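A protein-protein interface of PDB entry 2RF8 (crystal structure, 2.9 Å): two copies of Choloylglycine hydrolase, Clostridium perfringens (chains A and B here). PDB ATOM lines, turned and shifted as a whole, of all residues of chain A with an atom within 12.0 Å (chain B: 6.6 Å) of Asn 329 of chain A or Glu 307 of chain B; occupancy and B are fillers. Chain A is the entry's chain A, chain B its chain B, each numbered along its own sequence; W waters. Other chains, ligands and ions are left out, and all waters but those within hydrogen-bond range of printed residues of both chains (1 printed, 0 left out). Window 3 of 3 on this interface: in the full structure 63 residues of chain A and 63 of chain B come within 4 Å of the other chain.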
ATOM      1  N   ILE A 325      -1.032  10.678  19.111  1.00  0.00           N
ATOM      2  CA  ILE A 325      -1.795  10.605  17.868  1.00  0.00           C
ATOM      3  C   ILE A 325      -3.289  10.407  18.146  1.00  0.00           C
ATOM      4  O   ILE A 325      -3.671   9.612  19.006  1.00  0.00           O
ATOM      5  CB  ILE A 325      -1.266   9.479  16.929  1.00  0.00           C
ATOM      6  CG1 ILE A 325       0.226   9.658  16.627  1.00  0.00           C
ATOM      7  CG2 ILE A 325      -2.030   9.448  15.615  1.00  0.00           C
ATOM      8  CD1 ILE A 325       1.135   8.730  17.414  1.00  0.00           C
ATOM      9  N   ASN A 326      -4.122  11.149  17.420  1.00  0.00           N
ATOM     10  CA  ASN A 326      -5.567  10.960  17.457  1.00  0.00           C
ATOM     11  C   ASN A 326      -5.994   9.904  16.441  1.00  0.00           C
ATOM     12  O   ASN A 326      -5.829  10.091  15.234  1.00  0.00           O
ATOM     13  CB  ASN A 326      -6.293  12.282  17.193  1.00  0.00           C
ATOM     14  CG  ASN A 326      -7.787  12.102  16.977  1.00  0.00           C
ATOM     15  OD1 ASN A 326      -8.478  11.493  17.796  1.00  0.00           O
ATOM     16  ND2 ASN A 326      -8.291  12.637  15.873  1.00  0.00           N
ATOM     17  N   HIS A 327      -6.540   8.797  16.937  1.00  0.00           N
ATOM     18  CA  HIS A 327      -6.987   7.700  16.079  1.00  0.00           C
ATOM     19  C   HIS A 327      -8.435   7.921  15.642  1.00  0.00           C
ATOM     20  O   HIS A 327      -9.360   7.854  16.458  1.00  0.00           O
ATOM     21  CB  HIS A 327      -6.814   6.355  16.791  1.00  0.00           C
ATOM     22  CG  HIS A 327      -5.389   6.017  17.103  1.00  0.00           C
ATOM     23  ND1 HIS A 327      -4.654   5.125  16.352  1.00  0.00           N
ATOM     24  CD2 HIS A 327      -4.561   6.456  18.080  1.00  0.00           C
ATOM     25  CE1 HIS A 327      -3.436   5.025  16.855  1.00  0.00           C
ATOM     26  NE2 HIS A 327      -3.353   5.825  17.904  1.00  0.00           N
ATOM     27  N   VAL A 328      -8.616   8.188  14.351  1.00  0.00           N
ATOM     28  CA  VAL A 328      -9.911   8.606  13.805  1.00  0.00           C
ATOM     29  C   VAL A 328     -10.893   7.437  13.667  1.00  0.00           C
ATOM     30  O   VAL A 328     -12.092   7.594  13.916  1.00  0.00           O
ATOM     31  CB  VAL A 328      -9.738   9.356  12.450  1.00  0.00           C
ATOM     32  CG1 VAL A 328     -11.082   9.826  11.897  1.00  0.00           C
ATOM     33  CG2 VAL A 328      -8.795  10.546  12.611  1.00  0.00           C
ATOM     34  N   ASN A 329     -10.383   6.272  13.276  1.00  0.00           N
ATOM     35  CA  ASN A 329     -11.214   5.077  13.146  1.00  0.00           C
ATOM     36  C   ASN A 329     -10.647   3.881  13.909  1.00  0.00           C
ATOM     37  O   ASN A 329      -9.498   3.905  14.353  1.00  0.00           O
ATOM     38  CB  ASN A 329     -11.451   4.732  11.668  1.00  0.00           C
ATOM     39  CG  ASN A 329     -10.216   4.161  10.980  1.00  0.00           C
ATOM     40  OD1 ASN A 329      -9.079   4.422  11.382  1.00  0.00           O
ATOM     41  ND2 ASN A 329     -10.441   3.379   9.930  1.00  0.00           N
ATOM     42  OXT ASN A 329     -11.323   2.867  14.100  1.00  0.00           O
ATOM     43  N   PHE B  32     -12.152   6.582   1.482  1.00  0.00           N
ATOM     44  CA  PHE B  32     -11.794   5.168   1.495  1.00  0.00           C
ATOM     45  C   PHE B  32     -12.625   4.403   0.467  1.00  0.00           C
ATOM     46  O   PHE B  32     -13.852   4.518   0.442  1.00  0.00           O
ATOM     47  CB  PHE B  32     -11.983   4.579   2.897  1.00  0.00           C
ATOM     48  CG  PHE B  32     -11.851   3.080   2.955  1.00  0.00           C
ATOM     49  CD1 PHE B  32     -10.600   2.473   2.866  1.00  0.00           C
ATOM     50  CD2 PHE B  32     -12.977   2.276   3.111  1.00  0.00           C
ATOM     51  CE1 PHE B  32     -10.475   1.085   2.922  1.00  0.00           C
ATOM     52  CE2 PHE B  32     -12.862   0.889   3.170  1.00  0.00           C
ATOM     53  CZ  PHE B  32     -11.610   0.293   3.075  1.00  0.00           C
ATOM     54  N   ALA B 301      -4.679   9.782  12.768  1.00  0.00           N
ATOM     55  CA  ALA B 301      -4.422   8.504  12.107  1.00  0.00           C
ATOM     56  C   ALA B 301      -5.694   7.830  11.613  1.00  0.00           C
ATOM     57  O   ALA B 301      -6.681   7.717  12.345  1.00  0.00           O
ATOM     58  CB  ALA B 301      -3.650   7.571  13.027  1.00  0.00           C
ATOM     59  N   ILE B 302      -5.655   7.387  10.360  1.00  0.00           N
ATOM     60  CA  ILE B 302      -6.750   6.633   9.762  1.00  0.00           C
ATOM     61  C   ILE B 302      -6.185   5.339   9.178  1.00  0.00           C
ATOM     62  O   ILE B 302      -5.540   5.345   8.130  1.00  0.00           O
ATOM     63  CB  ILE B 302      -7.501   7.462   8.689  1.00  0.00           C
ATOM     64  CG1 ILE B 302      -8.039   8.755   9.305  1.00  0.00           C
ATOM     65  CG2 ILE B 302      -8.646   6.651   8.079  1.00  0.00           C
ATOM     66  CD1 ILE B 302      -8.121   9.917   8.351  1.00  0.00           C
ATOM     67  N   ASP B 303      -6.417   4.240   9.892  1.00  0.00           N
ATOM     68  CA  ASP B 303      -5.944   2.918   9.489  1.00  0.00           C
ATOM     69  C   ASP B 303      -6.981   2.270   8.579  1.00  0.00           C
ATOM     70  O   ASP B 303      -8.148   2.133   8.956  1.00  0.00           O
ATOM     71  CB  ASP B 303      -5.696   2.046  10.728  1.00  0.00           C
ATOM     72  CG  ASP B 303      -4.794   0.847  10.448  1.00  0.00           C
ATOM     73  OD1 ASP B 303      -4.879   0.251   9.352  1.00  0.00           O
ATOM     74  OD2 ASP B 303      -3.999   0.490  11.344  1.00  0.00           O
ATOM     75  N   MET B 304      -6.552   1.881   7.380  1.00  0.00           N
ATOM     76  CA  MET B 304      -7.453   1.250   6.417  1.00  0.00           C
ATOM     77  C   MET B 304      -7.746  -0.208   6.774  1.00  0.00           C
ATOM     78  O   MET B 304      -8.791  -0.744   6.400  1.00  0.00           O
ATOM     79  CB  MET B 304      -6.913   1.378   4.986  1.00  0.00           C
ATOM     80  CG  MET B 304      -5.869   0.344   4.578  1.00  0.00           C
ATOM     81  SD  MET B 304      -5.162   0.663   2.950  1.00  0.00           S
ATOM     82  CE  MET B 304      -6.632   0.795   1.941  1.00  0.00           C
ATOM     83  N   ASN B 305      -6.826  -0.837   7.505  1.00  0.00           N
ATOM     84  CA  ASN B 305      -6.986  -2.226   7.938  1.00  0.00           C
ATOM     85  C   ASN B 305      -8.067  -2.409   9.007  1.00  0.00           C
ATOM     86  O   ASN B 305      -8.551  -3.521   9.227  1.00  0.00           O
ATOM     87  CB  ASN B 305      -5.648  -2.801   8.412  1.00  0.00           C
ATOM     88  CG  ASN B 305      -4.622  -2.895   7.295  1.00  0.00           C
ATOM     89  OD1 ASN B 305      -4.906  -3.406   6.210  1.00  0.00           O
ATOM     90  ND2 ASN B 305      -3.417  -2.407   7.560  1.00  0.00           N
ATOM     91  N   LYS B 306      -8.441  -1.311   9.662  1.00  0.00           N
ATOM     92  CA  LYS B 306      -9.534  -1.318  10.633  1.00  0.00           C
ATOM     93  C   LYS B 306     -10.905  -1.344   9.947  1.00  0.00           C
ATOM     94  O   LYS B 306     -11.928  -1.587  10.592  1.00  0.00           O
ATOM     95  CB  LYS B 306      -9.426  -0.120  11.579  1.00  0.00           C
ATOM     96  CG  LYS B 306      -8.290  -0.238  12.582  1.00  0.00           C
ATOM     97  CD  LYS B 306      -8.493   0.693  13.756  1.00  0.00           C
ATOM     98  CE  LYS B 306      -7.544   0.355  14.889  1.00  0.00           C
ATOM     99  NZ  LYS B 306      -7.893   1.109  16.125  1.00  0.00           N
ATOM    100  N   GLU B 307     -10.910  -1.097   8.639  1.00  0.00           N
ATOM    101  CA  GLU B 307     -12.124  -1.160   7.836  1.00  0.00           C
ATOM    102  C   GLU B 307     -12.262  -2.516   7.154  1.00  0.00           C
ATOM    103  O   GLU B 307     -11.285  -3.257   7.020  1.00  0.00           O
ATOM    104  CB  GLU B 307     -12.128  -0.049   6.780  1.00  0.00           C
ATOM    105  CG  GLU B 307     -12.212   1.367   7.343  1.00  0.00           C
ATOM    106  CD  GLU B 307     -13.573   1.707   7.938  1.00  0.00           C
ATOM    107  OE1 GLU B 307     -14.521   0.902   7.802  1.00  0.00           O
ATOM    108  OE2 GLU B 307     -13.695   2.792   8.548  1.00  0.00           O
ATOM    109  N   ASN B 308     -13.484  -2.838   6.733  1.00  0.00           N
ATOM    110  CA  ASN B 308     -13.719  -4.019   5.916  1.00  0.00           C
ATOM    111  C   ASN B 308     -13.266  -3.745   4.487  1.00  0.00           C
ATOM    112  O   ASN B 308     -13.917  -3.002   3.747  1.00  0.00           O
ATOM    113  CB  ASN B 308     -15.196  -4.432   5.956  1.00  0.00           C
ATOM    114  CG  ASN B 308     -15.472  -5.721   5.186  1.00  0.00           C
ATOM    115  OD1 ASN B 308     -14.596  -6.575   5.028  1.00  0.00           O
ATOM    116  ND2 ASN B 308     -16.703  -5.865   4.710  1.00  0.00           N
ATOM    117  N   LEU B 309     -12.137  -4.343   4.114  1.00  0.00           N
ATOM    118  CA  LEU B 309     -11.551  -4.154   2.786  1.00  0.00           C
ATOM    119  C   LEU B 309     -12.395  -4.803   1.686  1.00  0.00           C
ATOM    120  O   LEU B 309     -12.213  -4.515   0.501  1.00  0.00           O
ATOM    121  CB  LEU B 309     -10.105  -4.669   2.752  1.00  0.00           C
ATOM    122  CG  LEU B 309      -9.121  -4.066   3.765  1.00  0.00           C
ATOM    123  CD1 LEU B 309      -7.753  -4.721   3.652  1.00  0.00           C
ATOM    124  CD2 LEU B 309      -9.000  -2.553   3.611  1.00  0.00           C
ATOM    125  N   ASP B 310     -13.315  -5.676   2.094  1.00  0.00           N
ATOM    126  CA  ASP B 310     -14.286  -6.276   1.185  1.00  0.00           C
ATOM    127  C   ASP B 310     -15.679  -5.670   1.378  1.00  0.00           C
ATOM    128  O   ASP B 310     -16.695  -6.350   1.221  1.00  0.00           O
ATOM    129  CB  ASP B 310     -14.319  -7.799   1.357  1.00  0.00           C
ATOM    130  CG  ASP B 310     -13.162  -8.492   0.659  1.00  0.00           C
ATOM    131  OD1 ASP B 310     -12.968  -8.269  -0.557  1.00  0.00           O
ATOM    132  OD2 ASP B 310     -12.450  -9.273   1.325  1.00  0.00           O
ATOM    133  N   LYS B 315     -16.291   5.001   2.221  1.00  0.00           N
ATOM    134  CA  LYS B 315     -16.338   5.603   3.552  1.00  0.00           C
ATOM    135  C   LYS B 315     -15.486   6.865   3.629  1.00  0.00           C
ATOM    136  O   LYS B 315     -14.349   6.885   3.152  1.00  0.00           O
ATOM    137  CB  LYS B 315     -15.904   4.597   4.620  1.00  0.00           C
ATOM    138  CG  LYS B 315     -16.900   3.464   4.836  1.00  0.00           C
ATOM    139  CD  LYS B 315     -16.625   2.694   6.121  1.00  0.00           C
ATOM    140  CE  LYS B 315     -17.041   3.485   7.359  1.00  0.00           C
ATOM    141  NZ  LYS B 315     -17.009   2.656   8.595  1.00  0.00           N
ATOM    142  N   TYR B 317     -14.160  10.429   6.073  1.00  0.00           N
ATOM    143  CA  TYR B 317     -13.853  10.952   7.401  1.00  0.00           C
ATOM    144  C   TYR B 317     -13.676  12.463   7.288  1.00  0.00           C
ATOM    145  O   TYR B 317     -13.032  12.941   6.352  1.00  0.00           O
ATOM    146  CB  TYR B 317     -12.574  10.311   7.950  1.00  0.00           C
ATOM    147  CG  TYR B 317     -12.517   8.804   7.808  1.00  0.00           C
ATOM    148  CD1 TYR B 317     -12.052   8.214   6.632  1.00  0.00           C
ATOM    149  CD2 TYR B 317     -12.922   7.967   8.849  1.00  0.00           C
ATOM    150  CE1 TYR B 317     -12.000   6.837   6.490  1.00  0.00           C
ATOM    151  CE2 TYR B 317     -12.869   6.581   8.719  1.00  0.00           C
ATOM    152  CZ  TYR B 317     -12.407   6.027   7.535  1.00  0.00           C
ATOM    153  OH  TYR B 317     -12.349   4.662   7.388  1.00  0.00           O
HETATM  154  O   HOH W   1      -7.205   5.185  13.241  1.00  0.00           O
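O of Asn 326 of chain A sits at hydrogen-bond distance from N of Ala 301 of chain B (2.7 Å).
The backbone NH (N) of Val 328 of chain A lies within hydrogen-bond range of the backbone carbonyl oxygen (O) of Ala 301 of chain B.
O of Asp 303 of chain B is in hydrogen-bond range of ND2 of Asn 329 of chain A, 2.8 Å away.
NZ of Lys 306 of chain B lies within salt-bridge range of O of Asn 329 of chain A, 3.7 Å away.
The side-chain amide nitrogen (ND2) of Asn 329 of chain A sits at hydrogen-bond distance from the side-chain hydroxyl (OH) of Tyr 317 of chain B, at 3.4 Å.
The backbone NH of Asn 305 of chain B is in hydrogen-bond range of the side-chain carboxylate of Asp 303 of chain B, 2.9 Å away.
OE1 of Glu 307 of chain B is in salt-bridge range of NZ of Lys 315 of chain B, at 3.1 Å.
OH of Tyr 317 of chain B lies within hydrogen-bond range of OE2 of Glu 307 of chain B, 2.6 Å away.
Ala 301 of chain B touches Ile 325 of chain A.
His 327 of chain A touches Ala 301 of chain B (C to O, 3.7 Å).
CG1 of Ile 302 of chain B touches CB of Val 328 of chain A (3.6 Å).
Asn 329 of chain A touches Ile 302 of chain B.
Asn 329 of chain A touches Glu 307 of chain B (ND2 to OE2, 3.6 Å).
Of the printed residues of chain B, His 327 of chain A touches Ala 301.
Printed residues of chain B within 4 Å of Asn 329 of chain A: Ile 302, Asp 303, Lys 306, Glu 307 and Tyr 317.
No residue of chain A comes within 4 Å of Phe 32 of chain B.
Printed residues of chain A within 4 Å of Ala 301 of chain B: Ile 325, Asn 326, His 327 and Val 328.
Of chain A, only Val 328 (3.6 Å) and Asn 329 (3.6 Å) come within 4 Å of Ile 302 of chain B.
Met 304 of chain B touches none of the printed residues of chain A.
Of chain A, only Asn 329 (3.4 Å) comes within 4 Å of Lys 306 of chain B.
Printed residues of chain A within 4 Å of Glu 307 of chain B: Asn 329.
No residue of chain A comes within 4 Å of Asn 308 of chain B.
No residue of chain A comes within 4 Å of Leu 309 of chain B.
Asp 310 of chain B touches none of the printed residues of chain A.
Printed residues of chain A within 4 Å of Tyr 317 of chain B: Asn 329 (3.4 Å).
The nearest residue of chain A that does not touch Glu 307 of chain B is Val 328 of chain A (7.4 Å).
The nearest printed residue of chain A that does not touch Tyr 317 of chain B is Val 328 of chain A (4.02 Å).
Along chain A the printed residues that touch a printed residue of chain B span positions 325 to 329.
No position is printed for both chains.
Of the 10 pairs that touch across the chains among the printed residues, none has its exchanged pair printed and touching as well.
Water W1 lies within hydrogen-bond range of O of Ala 301 of chain B, OD1 of Asn 329 of chain A and N of Val 328 of chain A.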
